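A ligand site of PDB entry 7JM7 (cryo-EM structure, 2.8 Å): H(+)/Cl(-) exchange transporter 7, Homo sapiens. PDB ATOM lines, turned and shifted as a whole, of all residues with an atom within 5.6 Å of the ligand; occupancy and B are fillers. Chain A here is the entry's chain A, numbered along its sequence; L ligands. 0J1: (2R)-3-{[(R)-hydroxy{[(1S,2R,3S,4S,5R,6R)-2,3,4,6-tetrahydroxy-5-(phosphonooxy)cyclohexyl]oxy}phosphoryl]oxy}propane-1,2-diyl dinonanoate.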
ATOM      1  N   LEU A 132     -24.835  -0.232   0.279  1.00  0.00           N
ATOM      2  CA  LEU A 132     -25.954  -0.929  -0.366  1.00  0.00           C
ATOM      3  C   LEU A 132     -25.899  -2.436  -0.135  1.00  0.00           C
ATOM      4  O   LEU A 132     -26.939  -3.063   0.086  1.00  0.00           O
ATOM      5  CB  LEU A 132     -25.998  -0.601  -1.857  1.00  0.00           C
ATOM      6  CG  LEU A 132     -26.643   0.697  -2.382  1.00  0.00           C
ATOM      7  CD1 LEU A 132     -27.132   1.613  -1.270  1.00  0.00           C
ATOM      8  CD2 LEU A 132     -25.718   1.475  -3.315  1.00  0.00           C
ATOM      9  N   LEU A 136     -29.057  -4.249   1.680  1.00  0.00           N
ATOM     10  CA  LEU A 136     -29.863  -5.243   0.989  1.00  0.00           C
ATOM     11  C   LEU A 136     -29.770  -6.604   1.664  1.00  0.00           C
ATOM     12  O   LEU A 136     -30.760  -7.333   1.741  1.00  0.00           O
ATOM     13  CB  LEU A 136     -29.436  -5.338  -0.473  1.00  0.00           C
ATOM     14  CG  LEU A 136     -29.680  -4.067  -1.297  1.00  0.00           C
ATOM     15  CD1 LEU A 136     -29.088  -4.217  -2.686  1.00  0.00           C
ATOM     16  CD2 LEU A 136     -31.152  -3.740  -1.382  1.00  0.00           C
ATOM     17  N   LEU A 139     -32.125  -6.403   4.571  1.00  0.00           N
ATOM     18  CA  LEU A 139     -33.521  -6.491   4.139  1.00  0.00           C
ATOM     19  C   LEU A 139     -33.885  -7.920   3.774  1.00  0.00           C
ATOM     20  O   LEU A 139     -34.992  -8.387   4.077  1.00  0.00           O
ATOM     21  CB  LEU A 139     -33.766  -5.554   2.955  1.00  0.00           C
ATOM     22  CG  LEU A 139     -33.662  -4.044   3.226  1.00  0.00           C
ATOM     23  CD1 LEU A 139     -34.282  -3.274   2.080  1.00  0.00           C
ATOM     24  CD2 LEU A 139     -34.305  -3.668   4.540  1.00  0.00           C
ATOM     25  N   VAL A 140     -32.983  -8.638   3.097  1.00  0.00           N
ATOM     26  CA  VAL A 140     -33.254 -10.021   2.741  1.00  0.00           C
ATOM     27  C   VAL A 140     -33.430 -10.874   3.999  1.00  0.00           C
ATOM     28  O   VAL A 140     -34.334 -11.714   4.073  1.00  0.00           O
ATOM     29  CB  VAL A 140     -32.129 -10.572   1.837  1.00  0.00           C
ATOM     30  CG1 VAL A 140     -32.120 -12.084   1.854  1.00  0.00           C
ATOM     31  CG2 VAL A 140     -32.287 -10.050   0.421  1.00  0.00           C
ATOM     32  N   ILE A 218     -17.212 -21.612  -9.446  1.00  0.00           N
ATOM     33  CA  ILE A 218     -18.190 -22.662  -9.718  1.00  0.00           C
ATOM     34  C   ILE A 218     -19.248 -22.031 -10.629  1.00  0.00           C
ATOM     35  O   ILE A 218     -19.586 -20.852 -10.438  1.00  0.00           O
ATOM     36  CB  ILE A 218     -18.775 -23.234  -8.417  1.00  0.00           C
ATOM     37  CG1 ILE A 218     -17.674 -23.987  -7.653  1.00  0.00           C
ATOM     38  CG2 ILE A 218     -19.920 -24.171  -8.691  1.00  0.00           C
ATOM     39  CD1 ILE A 218     -18.050 -24.392  -6.256  1.00  0.00           C
ATOM     40  N   PRO A 219     -19.780 -22.752 -11.611  1.00  0.00           N
ATOM     41  CA  PRO A 219     -20.413 -22.079 -12.755  1.00  0.00           C
ATOM     42  C   PRO A 219     -21.530 -21.098 -12.422  1.00  0.00           C
ATOM     43  O   PRO A 219     -21.585 -20.018 -13.014  1.00  0.00           O
ATOM     44  CB  PRO A 219     -20.931 -23.255 -13.597  1.00  0.00           C
ATOM     45  CG  PRO A 219     -20.003 -24.358 -13.289  1.00  0.00           C
ATOM     46  CD  PRO A 219     -19.690 -24.214 -11.837  1.00  0.00           C
ATOM     47  N   HIS A 220     -22.428 -21.431 -11.497  1.00  0.00           N
ATOM     48  CA  HIS A 220     -23.644 -20.638 -11.268  1.00  0.00           C
ATOM     49  C   HIS A 220     -23.788 -20.251  -9.808  1.00  0.00           C
ATOM     50  O   HIS A 220     -24.839 -20.442  -9.184  1.00  0.00           O
ATOM     51  CB  HIS A 220     -24.903 -21.385 -11.721  1.00  0.00           C
ATOM     52  CG  HIS A 220     -24.746 -22.092 -13.033  1.00  0.00           C
ATOM     53  ND1 HIS A 220     -24.805 -21.436 -14.244  1.00  0.00           N
ATOM     54  CD2 HIS A 220     -24.577 -23.402 -13.317  1.00  0.00           C
ATOM     55  CE1 HIS A 220     -24.655 -22.314 -15.218  1.00  0.00           C
ATOM     56  NE2 HIS A 220     -24.515 -23.513 -14.683  1.00  0.00           N
ATOM     57  N   VAL A 221     -22.737 -19.682  -9.220  1.00  0.00           N
ATOM     58  CA  VAL A 221     -22.779 -19.352  -7.797  1.00  0.00           C
ATOM     59  C   VAL A 221     -23.371 -17.974  -7.521  1.00  0.00           C
ATOM     60  O   VAL A 221     -24.029 -17.787  -6.491  1.00  0.00           O
ATOM     61  CB  VAL A 221     -21.371 -19.469  -7.180  1.00  0.00           C
ATOM     62  CG1 VAL A 221     -20.974 -20.914  -7.056  1.00  0.00           C
ATOM     63  CG2 VAL A 221     -20.349 -18.693  -7.999  1.00  0.00           C
ATOM     64  N   VAL A 222     -23.160 -17.012  -8.413  1.00  0.00           N
ATOM     65  CA  VAL A 222     -23.529 -15.620  -8.129  1.00  0.00           C
ATOM     66  C   VAL A 222     -24.599 -15.139  -9.098  1.00  0.00           C
ATOM     67  O   VAL A 222     -24.618 -13.960  -9.484  1.00  0.00           O
ATOM     68  CB  VAL A 222     -22.291 -14.701  -8.172  1.00  0.00           C
ATOM     69  CG1 VAL A 222     -21.379 -14.988  -7.005  1.00  0.00           C
ATOM     70  CG2 VAL A 222     -21.557 -14.868  -9.487  1.00  0.00           C
ATOM     71  N   ARG A 223     -25.488 -16.032  -9.514  1.00  0.00           N
ATOM     72  CA  ARG A 223     -26.563 -15.691 -10.430  1.00  0.00           C
ATOM     73  C   ARG A 223     -27.832 -15.310  -9.684  1.00  0.00           C
ATOM     74  O   ARG A 223     -28.071 -15.751  -8.549  1.00  0.00           O
ATOM     75  CB  ARG A 223     -26.838 -16.850 -11.381  1.00  0.00           C
ATOM     76  CG  ARG A 223     -25.628 -17.309 -12.155  1.00  0.00           C
ATOM     77  CD  ARG A 223     -25.990 -17.724 -13.576  1.00  0.00           C
ATOM     78  NE  ARG A 223     -24.861 -18.336 -14.268  1.00  0.00           N
ATOM     79  CZ  ARG A 223     -24.877 -18.664 -15.554  1.00  0.00           C
ATOM     80  NH1 ARG A 223     -25.939 -18.429 -16.297  1.00  0.00           N
ATOM     81  NH2 ARG A 223     -23.800 -19.224 -16.098  1.00  0.00           N
ATOM     82  N   LEU A 224     -28.643 -14.471 -10.323  1.00  0.00           N
ATOM     83  CA  LEU A 224     -29.912 -14.035  -9.719  1.00  0.00           C
ATOM     84  C   LEU A 224     -30.843 -15.218  -9.476  1.00  0.00           C
ATOM     85  O   LEU A 224     -31.485 -15.310  -8.423  1.00  0.00           O
ATOM     86  CB  LEU A 224     -30.581 -13.012 -10.632  1.00  0.00           C
ATOM     87  CG  LEU A 224     -31.960 -12.509 -10.214  1.00  0.00           C
ATOM     88  CD1 LEU A 224     -31.878 -11.754  -8.898  1.00  0.00           C
ATOM     89  CD2 LEU A 224     -32.532 -11.623 -11.306  1.00  0.00           C
ATOM     90  N   LYS A 225     -30.925 -16.123 -10.451  1.00  0.00           N
ATOM     91  CA  LYS A 225     -31.743 -17.314 -10.281  1.00  0.00           C
ATOM     92  C   LYS A 225     -31.349 -18.068  -9.029  1.00  0.00           C
ATOM     93  O   LYS A 225     -32.193 -18.568  -8.290  1.00  0.00           O
ATOM     94  CB  LYS A 225     -31.623 -18.207 -11.522  1.00  0.00           C
ATOM     95  CG  LYS A 225     -32.508 -19.435 -11.515  1.00  0.00           C
ATOM     96  CD  LYS A 225     -32.114 -20.396 -12.611  1.00  0.00           C
ATOM     97  CE  LYS A 225     -32.759 -20.025 -13.928  1.00  0.00           C
ATOM     98  NZ  LYS A 225     -32.503 -21.060 -14.976  1.00  0.00           N
ATOM     99  N   LEU A 227     -30.024 -16.825  -6.287  1.00  0.00           N
ATOM    100  CA  LEU A 227     -30.501 -16.087  -5.115  1.00  0.00           C
ATOM    101  C   LEU A 227     -31.980 -16.359  -4.873  1.00  0.00           C
ATOM    102  O   LEU A 227     -32.385 -16.694  -3.752  1.00  0.00           O
ATOM    103  CB  LEU A 227     -30.262 -14.588  -5.313  1.00  0.00           C
ATOM    104  CG  LEU A 227     -30.686 -13.673  -4.157  1.00  0.00           C
ATOM    105  CD1 LEU A 227     -29.980 -14.059  -2.878  1.00  0.00           C
ATOM    106  CD2 LEU A 227     -30.419 -12.223  -4.499  1.00  0.00           C
ATOM    107  N   VAL A 256     -23.981 -13.007  -3.583  1.00  0.00           N
ATOM    108  CA  VAL A 256     -24.658 -12.759  -4.858  1.00  0.00           C
ATOM    109  C   VAL A 256     -24.904 -11.269  -5.028  1.00  0.00           C
ATOM    110  O   VAL A 256     -24.525 -10.665  -6.033  1.00  0.00           O
ATOM    111  CB  VAL A 256     -25.971 -13.549  -4.938  1.00  0.00           C
ATOM    112  CG1 VAL A 256     -26.728 -13.177  -6.193  1.00  0.00           C
ATOM    113  CG2 VAL A 256     -25.709 -15.043  -4.914  1.00  0.00           C
ATOM    114  N   ILE A 257     -25.467 -10.645  -3.997  1.00  0.00           N
ATOM    115  CA  ILE A 257     -25.776  -9.224  -4.094  1.00  0.00           C
ATOM    116  C   ILE A 257     -24.511  -8.442  -4.418  1.00  0.00           C
ATOM    117  O   ILE A 257     -24.484  -7.614  -5.333  1.00  0.00           O
ATOM    118  CB  ILE A 257     -26.438  -8.725  -2.799  1.00  0.00           C
ATOM    119  CG1 ILE A 257     -27.768  -9.458  -2.566  1.00  0.00           C
ATOM    120  CG2 ILE A 257     -26.674  -7.235  -2.853  1.00  0.00           C
ATOM    121  CD1 ILE A 257     -28.235  -9.430  -1.132  1.00  0.00           C
ATOM    122  N   ALA A 259     -21.832  -9.450  -5.886  1.00  0.00           N
ATOM    123  CA  ALA A 259     -21.407  -9.706  -7.249  1.00  0.00           C
ATOM    124  C   ALA A 259     -22.341  -9.072  -8.265  1.00  0.00           C
ATOM    125  O   ALA A 259     -21.931  -8.874  -9.418  1.00  0.00           O
ATOM    126  CB  ALA A 259     -21.322 -11.218  -7.486  1.00  0.00           C
ATOM    127  N   GLY A 260     -23.576  -8.759  -7.883  1.00  0.00           N
ATOM    128  CA  GLY A 260     -24.545  -8.247  -8.834  1.00  0.00           C
ATOM    129  C   GLY A 260     -24.546  -6.746  -8.977  1.00  0.00           C
ATOM    130  O   GLY A 260     -24.376  -6.217 -10.077  1.00  0.00           O
ATOM    131  N   ILE A 261     -24.740  -6.038  -7.858  1.00  0.00           N
ATOM    132  CA  ILE A 261     -24.851  -4.585  -7.918  1.00  0.00           C
ATOM    133  C   ILE A 261     -23.506  -3.941  -8.220  1.00  0.00           C
ATOM    134  O   ILE A 261     -23.468  -2.777  -8.660  1.00  0.00           O
ATOM    135  CB  ILE A 261     -25.439  -4.045  -6.603  1.00  0.00           C
ATOM    136  CG1 ILE A 261     -24.488  -4.308  -5.433  1.00  0.00           C
ATOM    137  CG2 ILE A 261     -26.788  -4.688  -6.318  1.00  0.00           C
ATOM    138  CD1 ILE A 261     -24.909  -3.625  -4.149  1.00  0.00           C
ATOM    139  N   GLN A 263     -21.419  -4.783 -10.611  1.00  0.00           N
ATOM    140  CA  GLN A 263     -21.228  -4.684 -12.052  1.00  0.00           C
ATOM    141  C   GLN A 263     -22.060  -3.563 -12.666  1.00  0.00           C
ATOM    142  O   GLN A 263     -21.717  -3.084 -13.752  1.00  0.00           O
ATOM    143  CB  GLN A 263     -21.577  -5.999 -12.726  1.00  0.00           C
ATOM    144  CG  GLN A 263     -20.871  -7.204 -12.132  1.00  0.00           C
ATOM    145  CD  GLN A 263     -19.367  -7.067 -12.174  1.00  0.00           C
ATOM    146  OE1 GLN A 263     -18.791  -6.738 -13.209  1.00  0.00           O
ATOM    147  NE2 GLN A 263     -18.720  -7.307 -11.046  1.00  0.00           N
ATOM    148  N   GLY A 264     -23.126  -3.131 -12.001  1.00  0.00           N
ATOM    149  CA  GLY A 264     -23.964  -2.079 -12.532  1.00  0.00           C
ATOM    150  C   GLY A 264     -24.907  -2.501 -13.646  1.00  0.00           C
ATOM    151  O   GLY A 264     -25.451  -1.631 -14.335  1.00  0.00           O
ATOM    152  N   ARG A 265     -25.116  -3.796 -13.838  1.00  0.00           N
ATOM    153  CA  ARG A 265     -25.983  -4.276 -14.905  1.00  0.00           C
ATOM    154  C   ARG A 265     -26.485  -5.668 -14.551  1.00  0.00           C
ATOM    155  O   ARG A 265     -25.919  -6.351 -13.693  1.00  0.00           O
ATOM    156  CB  ARG A 265     -25.263  -4.299 -16.250  1.00  0.00           C
ATOM    157  CG  ARG A 265     -24.066  -5.236 -16.317  1.00  0.00           C
ATOM    158  CD  ARG A 265     -23.455  -5.246 -17.707  1.00  0.00           C
ATOM    159  NE  ARG A 265     -22.152  -5.889 -17.718  1.00  0.00           N
ATOM    160  CZ  ARG A 265     -21.349  -5.938 -18.785  1.00  0.00           C
ATOM    161  NH1 ARG A 265     -21.715  -5.371 -19.921  1.00  0.00           N
ATOM    162  NH2 ARG A 265     -20.175  -6.542 -18.701  1.00  0.00           N
ATOM    163  N   SER A 266     -27.564  -6.071 -15.225  1.00  0.00           N
ATOM    164  CA  SER A 266     -28.176  -7.380 -15.033  1.00  0.00           C
ATOM    165  C   SER A 266     -28.010  -8.187 -16.325  1.00  0.00           C
ATOM    166  O   SER A 266     -28.731  -7.971 -17.300  1.00  0.00           O
ATOM    167  CB  SER A 266     -29.646  -7.251 -14.647  1.00  0.00           C
ATOM    168  OG  SER A 266     -30.210  -8.522 -14.377  1.00  0.00           O
ATOM    169  N   THR A 267     -27.054  -9.114 -16.324  1.00  0.00           N
ATOM    170  CA  THR A 267     -26.864  -9.979 -17.479  1.00  0.00           C
ATOM    171  C   THR A 267     -28.071 -10.885 -17.691  1.00  0.00           C
ATOM    172  O   THR A 267     -28.518 -11.063 -18.828  1.00  0.00           O
ATOM    173  CB  THR A 267     -25.594 -10.813 -17.306  1.00  0.00           C
ATOM    174  OG1 THR A 267     -24.488  -9.950 -17.029  1.00  0.00           O
ATOM    175  CG2 THR A 267     -25.305 -11.628 -18.554  1.00  0.00           C
ATOM    176  N   SER A 268     -28.608 -11.467 -16.614  1.00  0.00           N
ATOM    177  CA  SER A 268     -29.731 -12.383 -16.751  1.00  0.00           C
ATOM    178  C   SER A 268     -30.958 -11.667 -17.314  1.00  0.00           C
ATOM    179  O   SER A 268     -31.644 -12.195 -18.187  1.00  0.00           O
ATOM    180  CB  SER A 268     -30.055 -13.023 -15.398  1.00  0.00           C
ATOM    181  OG  SER A 268     -28.909 -13.671 -14.863  1.00  0.00           O
ATOM    182  N   LEU A 269     -31.242 -10.467 -16.809  1.00  0.00           N
ATOM    183  CA  LEU A 269     -32.380  -9.697 -17.285  1.00  0.00           C
ATOM    184  C   LEU A 269     -32.050  -8.835 -18.501  1.00  0.00           C
ATOM    185  O   LEU A 269     -32.968  -8.223 -19.071  1.00  0.00           O
ATOM    186  CB  LEU A 269     -32.907  -8.798 -16.165  1.00  0.00           C
ATOM    187  CG  LEU A 269     -33.159  -9.475 -14.811  1.00  0.00           C
ATOM    188  CD1 LEU A 269     -33.672  -8.465 -13.799  1.00  0.00           C
ATOM    189  CD2 LEU A 269     -34.135 -10.631 -14.961  1.00  0.00           C
ATOM    190  N   PHE A 273     -27.571  -0.512 -16.519  1.00  0.00           N
ATOM    191  CA  PHE A 273     -27.571   0.852 -16.013  1.00  0.00           C
ATOM    192  C   PHE A 273     -26.149   1.412 -16.061  1.00  0.00           C
ATOM    193  O   PHE A 273     -25.176   0.695 -15.831  1.00  0.00           O
ATOM    194  CB  PHE A 273     -28.106   0.946 -14.579  1.00  0.00           C
ATOM    195  CG  PHE A 273     -29.568   0.605 -14.460  1.00  0.00           C
ATOM    196  CD1 PHE A 273     -30.533   1.504 -14.868  1.00  0.00           C
ATOM    197  CD2 PHE A 273     -29.965  -0.574 -13.866  1.00  0.00           C
ATOM    198  CE1 PHE A 273     -31.872   1.205 -14.753  1.00  0.00           C
ATOM    199  CE2 PHE A 273     -31.312  -0.879 -13.732  1.00  0.00           C
ATOM    200  CZ  PHE A 273     -32.268   0.019 -14.171  1.00  0.00           C
ATOM    201  N   ILE A 275     -23.701   2.848 -14.564  1.00  0.00           N
ATOM    202  CA  ILE A 275     -22.886   3.108 -13.380  1.00  0.00           C
ATOM    203  C   ILE A 275     -21.974   1.914 -13.141  1.00  0.00           C
ATOM    204  O   ILE A 275     -22.226   0.811 -13.610  1.00  0.00           O
ATOM    205  CB  ILE A 275     -23.738   3.410 -12.121  1.00  0.00           C
ATOM    206  CG1 ILE A 275     -24.620   2.209 -11.765  1.00  0.00           C
ATOM    207  CG2 ILE A 275     -24.572   4.652 -12.336  1.00  0.00           C
ATOM    208  CD1 ILE A 275     -25.282   2.339 -10.409  1.00  0.00           C
ATOM    209  N   PHE A 276     -20.912   2.164 -12.381  1.00  0.00           N
ATOM    210  CA  PHE A 276     -20.014   1.103 -11.918  1.00  0.00           C
ATOM    211  C   PHE A 276     -19.395   0.334 -13.082  1.00  0.00           C
ATOM    212  O   PHE A 276     -19.273  -0.893 -13.028  1.00  0.00           O
ATOM    213  CB  PHE A 276     -20.741   0.150 -10.961  1.00  0.00           C
ATOM    214  CG  PHE A 276     -21.364   0.814  -9.774  1.00  0.00           C
ATOM    215  CD1 PHE A 276     -20.992   2.093  -9.384  1.00  0.00           C
ATOM    216  CD2 PHE A 276     -22.328   0.158  -9.026  1.00  0.00           C
ATOM    217  CE1 PHE A 276     -21.571   2.699  -8.284  1.00  0.00           C
ATOM    218  CE2 PHE A 276     -22.913   0.758  -7.931  1.00  0.00           C
ATOM    219  CZ  PHE A 276     -22.534   2.029  -7.560  1.00  0.00           C
ATOM    220  N   LYS A 285     -14.706  -7.536  -7.865  1.00  0.00           N
ATOM    221  CA  LYS A 285     -15.764  -8.510  -7.615  1.00  0.00           C
ATOM    222  C   LYS A 285     -15.460  -9.338  -6.379  1.00  0.00           C
ATOM    223  O   LYS A 285     -16.332  -9.526  -5.517  1.00  0.00           O
ATOM    224  CB  LYS A 285     -15.932  -9.402  -8.842  1.00  0.00           C
ATOM    225  CG  LYS A 285     -17.258 -10.112  -8.930  1.00  0.00           C
ATOM    226  CD  LYS A 285     -17.411 -10.809 -10.277  1.00  0.00           C
ATOM    227  CE  LYS A 285     -18.531 -11.829 -10.250  1.00  0.00           C
ATOM    228  NZ  LYS A 285     -18.673 -12.497 -11.563  1.00  0.00           N
ATOM    229  N   PRO A 716     -18.872 -10.578 -17.960  1.00  0.00           N
ATOM    230  CA  PRO A 716     -17.921 -11.610 -17.521  1.00  0.00           C
ATOM    231  C   PRO A 716     -17.840 -12.793 -18.477  1.00  0.00           C
ATOM    232  O   PRO A 716     -17.050 -13.708 -18.248  1.00  0.00           O
ATOM    233  CB  PRO A 716     -18.491 -12.062 -16.168  1.00  0.00           C
ATOM    234  CG  PRO A 716     -19.518 -11.035 -15.802  1.00  0.00           C
ATOM    235  CD  PRO A 716     -20.073 -10.596 -17.116  1.00  0.00           C
ATOM    236  N   ARG A 717     -18.661 -12.786 -19.526  1.00  0.00           N
ATOM    237  CA  ARG A 717     -18.788 -13.906 -20.445  1.00  0.00           C
ATOM    238  C   ARG A 717     -18.139 -13.549 -21.769  1.00  0.00           C
ATOM    239  O   ARG A 717     -18.516 -12.543 -22.395  1.00  0.00           O
ATOM    240  CB  ARG A 717     -20.252 -14.280 -20.646  1.00  0.00           C
ATOM    241  CG  ARG A 717     -20.918 -14.865 -19.415  1.00  0.00           C
ATOM    242  CD  ARG A 717     -22.433 -14.746 -19.456  1.00  0.00           C
ATOM    243  NE  ARG A 717     -23.047 -15.259 -18.242  1.00  0.00           N
ATOM    244  CZ  ARG A 717     -24.354 -15.303 -18.025  1.00  0.00           C
ATOM    245  NH1 ARG A 717     -24.822 -15.794 -16.886  1.00  0.00           N
ATOM    246  NH2 ARG A 717     -25.205 -14.841 -18.932  1.00  0.00           N
HETATM  247  C02 0J1 L   1     -34.645  -7.088  -0.106  1.00  0.00           C
HETATM  248  C03 0J1 L   1     -34.181  -7.684  -1.416  1.00  0.00           C
HETATM  249  C04 0J1 L   1     -32.856  -7.091  -1.904  1.00  0.00           C
HETATM  250  C05 0J1 L   1     -32.018  -8.123  -2.665  1.00  0.00           C
HETATM  251  C06 0J1 L   1     -31.123  -7.508  -3.764  1.00  0.00           C
HETATM  252  C07 0J1 L   1     -30.969  -8.462  -4.965  1.00  0.00           C
HETATM  253  C08 0J1 L   1     -30.090  -7.887  -6.074  1.00  0.00           C
HETATM  254  C09 0J1 L   1     -28.771  -8.656  -6.255  1.00  0.00           C
HETATM  255  C10 0J1 L   1     -28.790  -9.687  -7.399  1.00  0.00           C
HETATM  256  C13 0J1 L   1     -28.460  -8.143  -9.200  1.00  0.00           C
HETATM  257  C14 0J1 L   1     -28.518  -8.335 -10.729  1.00  0.00           C
HETATM  258  C15 0J1 L   1     -27.181  -8.857 -11.303  1.00  0.00           C
HETATM  259  C21 0J1 L   1     -24.827 -11.861 -13.524  1.00  0.00           C
HETATM  260  C22 0J1 L   1     -23.787 -11.241 -12.578  1.00  0.00           C
HETATM  261  C24 0J1 L   1     -22.361 -11.738 -12.739  1.00  0.00           C
HETATM  262  C26 0J1 L   1     -22.311 -13.245 -12.915  1.00  0.00           C
HETATM  263  C28 0J1 L   1     -23.007 -13.636 -14.205  1.00  0.00           C
HETATM  264  C34 0J1 L   1     -24.458 -13.162 -14.263  1.00  0.00           C
HETATM  265  C37 0J1 L   1     -28.116  -5.959 -10.938  1.00  0.00           C
HETATM  266  C39 0J1 L   1     -28.853  -4.811 -10.211  1.00  0.00           C
HETATM  267  C40 0J1 L   1     -28.501  -3.412 -10.792  1.00  0.00           C
HETATM  268  C41 0J1 L   1     -27.308  -2.752 -10.064  1.00  0.00           C
HETATM  269  C42 0J1 L   1     -27.245  -1.217 -10.275  1.00  0.00           C
HETATM  270  C43 0J1 L   1     -27.809  -0.446  -9.076  1.00  0.00           C
HETATM  271  C44 0J1 L   1     -26.795  -0.326  -7.939  1.00  0.00           C
HETATM  272  C45 0J1 L   1     -27.456   0.024  -6.611  1.00  0.00           C
HETATM  273  C46 0J1 L   1     -27.788  -1.216  -5.777  1.00  0.00           C
HETATM  274  O11 0J1 L   1     -29.334 -10.720  -7.250  1.00  0.00           O
HETATM  275  O12 0J1 L   1     -28.156  -9.412  -8.632  1.00  0.00           O
HETATM  276  O16 0J1 L   1     -27.207 -10.257 -11.265  1.00  0.00           O
HETATM  277  O18 0J1 L   1     -28.512 -12.006 -12.649  1.00  0.00           O
HETATM  278  O19 0J1 L   1     -27.299 -10.257 -13.868  1.00  0.00           O
HETATM  279  O20 0J1 L   1     -25.953 -12.167 -12.724  1.00  0.00           O
HETATM  280  O23 0J1 L   1     -23.791  -9.862 -12.787  1.00  0.00           O
HETATM  281  O25 0J1 L   1     -21.637 -11.396 -11.593  1.00  0.00           O
HETATM  282  O27 0J1 L   1     -20.978 -13.649 -12.930  1.00  0.00           O
HETATM  283  O29 0J1 L   1     -23.022 -15.027 -14.306  1.00  0.00           O
HETATM  284  O31 0J1 L   1     -20.592 -14.865 -15.141  1.00  0.00           O
HETATM  285  O32 0J1 L   1     -21.132 -16.533 -13.430  1.00  0.00           O
HETATM  286  O33 0J1 L   1     -21.907 -16.855 -15.737  1.00  0.00           O
HETATM  287  O35 0J1 L   1     -25.255 -14.178 -13.736  1.00  0.00           O
HETATM  288  O36 0J1 L   1     -28.835  -7.109 -11.372  1.00  0.00           O
HETATM  289  O38 0J1 L   1     -26.950  -5.875 -11.152  1.00  0.00           O
HETATM  290  P17 0J1 L   1     -27.269 -11.159 -12.665  1.00  0.00           P
HETATM  291  P30 0J1 L   1     -21.640 -15.835 -14.668  1.00  0.00           P
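An oxygen (O19) of the ligand lies within hydrogen-bond range of the backbone NH (N) of Thr 267 (2.7 Å). The backbone NH (N) of Ser 268 is in hydrogen-bond range of an oxygen (O19) of the ligand (3.3 Å). An oxygen (O18) of the ligand sits at hydrogen-bond distance from the side-chain hydroxyl of Ser 268 (2.8 Å). An oxygen (O27) of the ligand sits at hydrogen-bond distance from the side-chain amino group (NZ) of Lys 285, 2.9 Å away. O33 of the ligand is in salt-bridge range of NH2 of Arg 223 (3.1 Å). An oxygen (O18) of the ligand sits close to the backbone NH (N) of Leu 224. An oxygen (O33) of the ligand is in salt-bridge range of the guanidinium group of Arg 717, 3.2 Å away. O19 of the ligand sits close to OG of Ser 266, at 3.4 Å. The backbone carbonyl oxygen of Ala 259 sits at hydrogen-bond distance from an oxygen (O25) of the ligand, 3.3 Å away.
The guanidinium group of Arg 223 sits at hydrogen-bond distance from a ring nitrogen (ND1) of His 220. OG of Ser 266 sits close to N of Leu 269.
O38 of the ligand sits close to O of Gly 260 (2.8 Å). O of Arg 265 lies close to O38 of the ligand, 2.8 Å away. Leu 132 touches the ligand. Leu 136 touches the ligand (CD2 to C04, 3.8 Å). CB of Leu 139 touches C02 of the ligand, 3.5 Å away. Val 140 touches the ligand. O of Pro 219 touches O32 of the ligand (3.5 Å). Val 222 touches the ligand. CD2 of Leu 227 touches O11 of the ligand, at 3.3 Å. Val 256 touches the ligand. CA of Ile 257 touches C09 of the ligand (3.7 Å). CG2 of Ile 261 touches C46 of the ligand (3.7 Å). CD1 of Ile 275 touches C44 of the ligand, 3.9 Å away. CB of Pro 716 touches O31 of the ligand (3.7 Å). Hydrophobic or aromatic side chains that line the ligand: Leu 132, Leu 136, Leu 139, Val 140, Val 222, Leu 224, Leu 227, Val 256, Ile 257, Ile 261, Ile 275 and Pro 716. Within 4 Å of the ligand: Leu 132, Leu 136, Leu 139, Val 140, Pro 219, Val 222, Arg 223, Leu 224, Leu 227, Val 256, Ile 257, Ala 259, Gly 260, Ile 261, Arg 265, Ser 266, Thr 267, Ser 268, Ile 275, Lys 285, Pro 716 and Arg 717. The nearest printed residue that does not touch the ligand is Gln 263 (4.003 Å).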
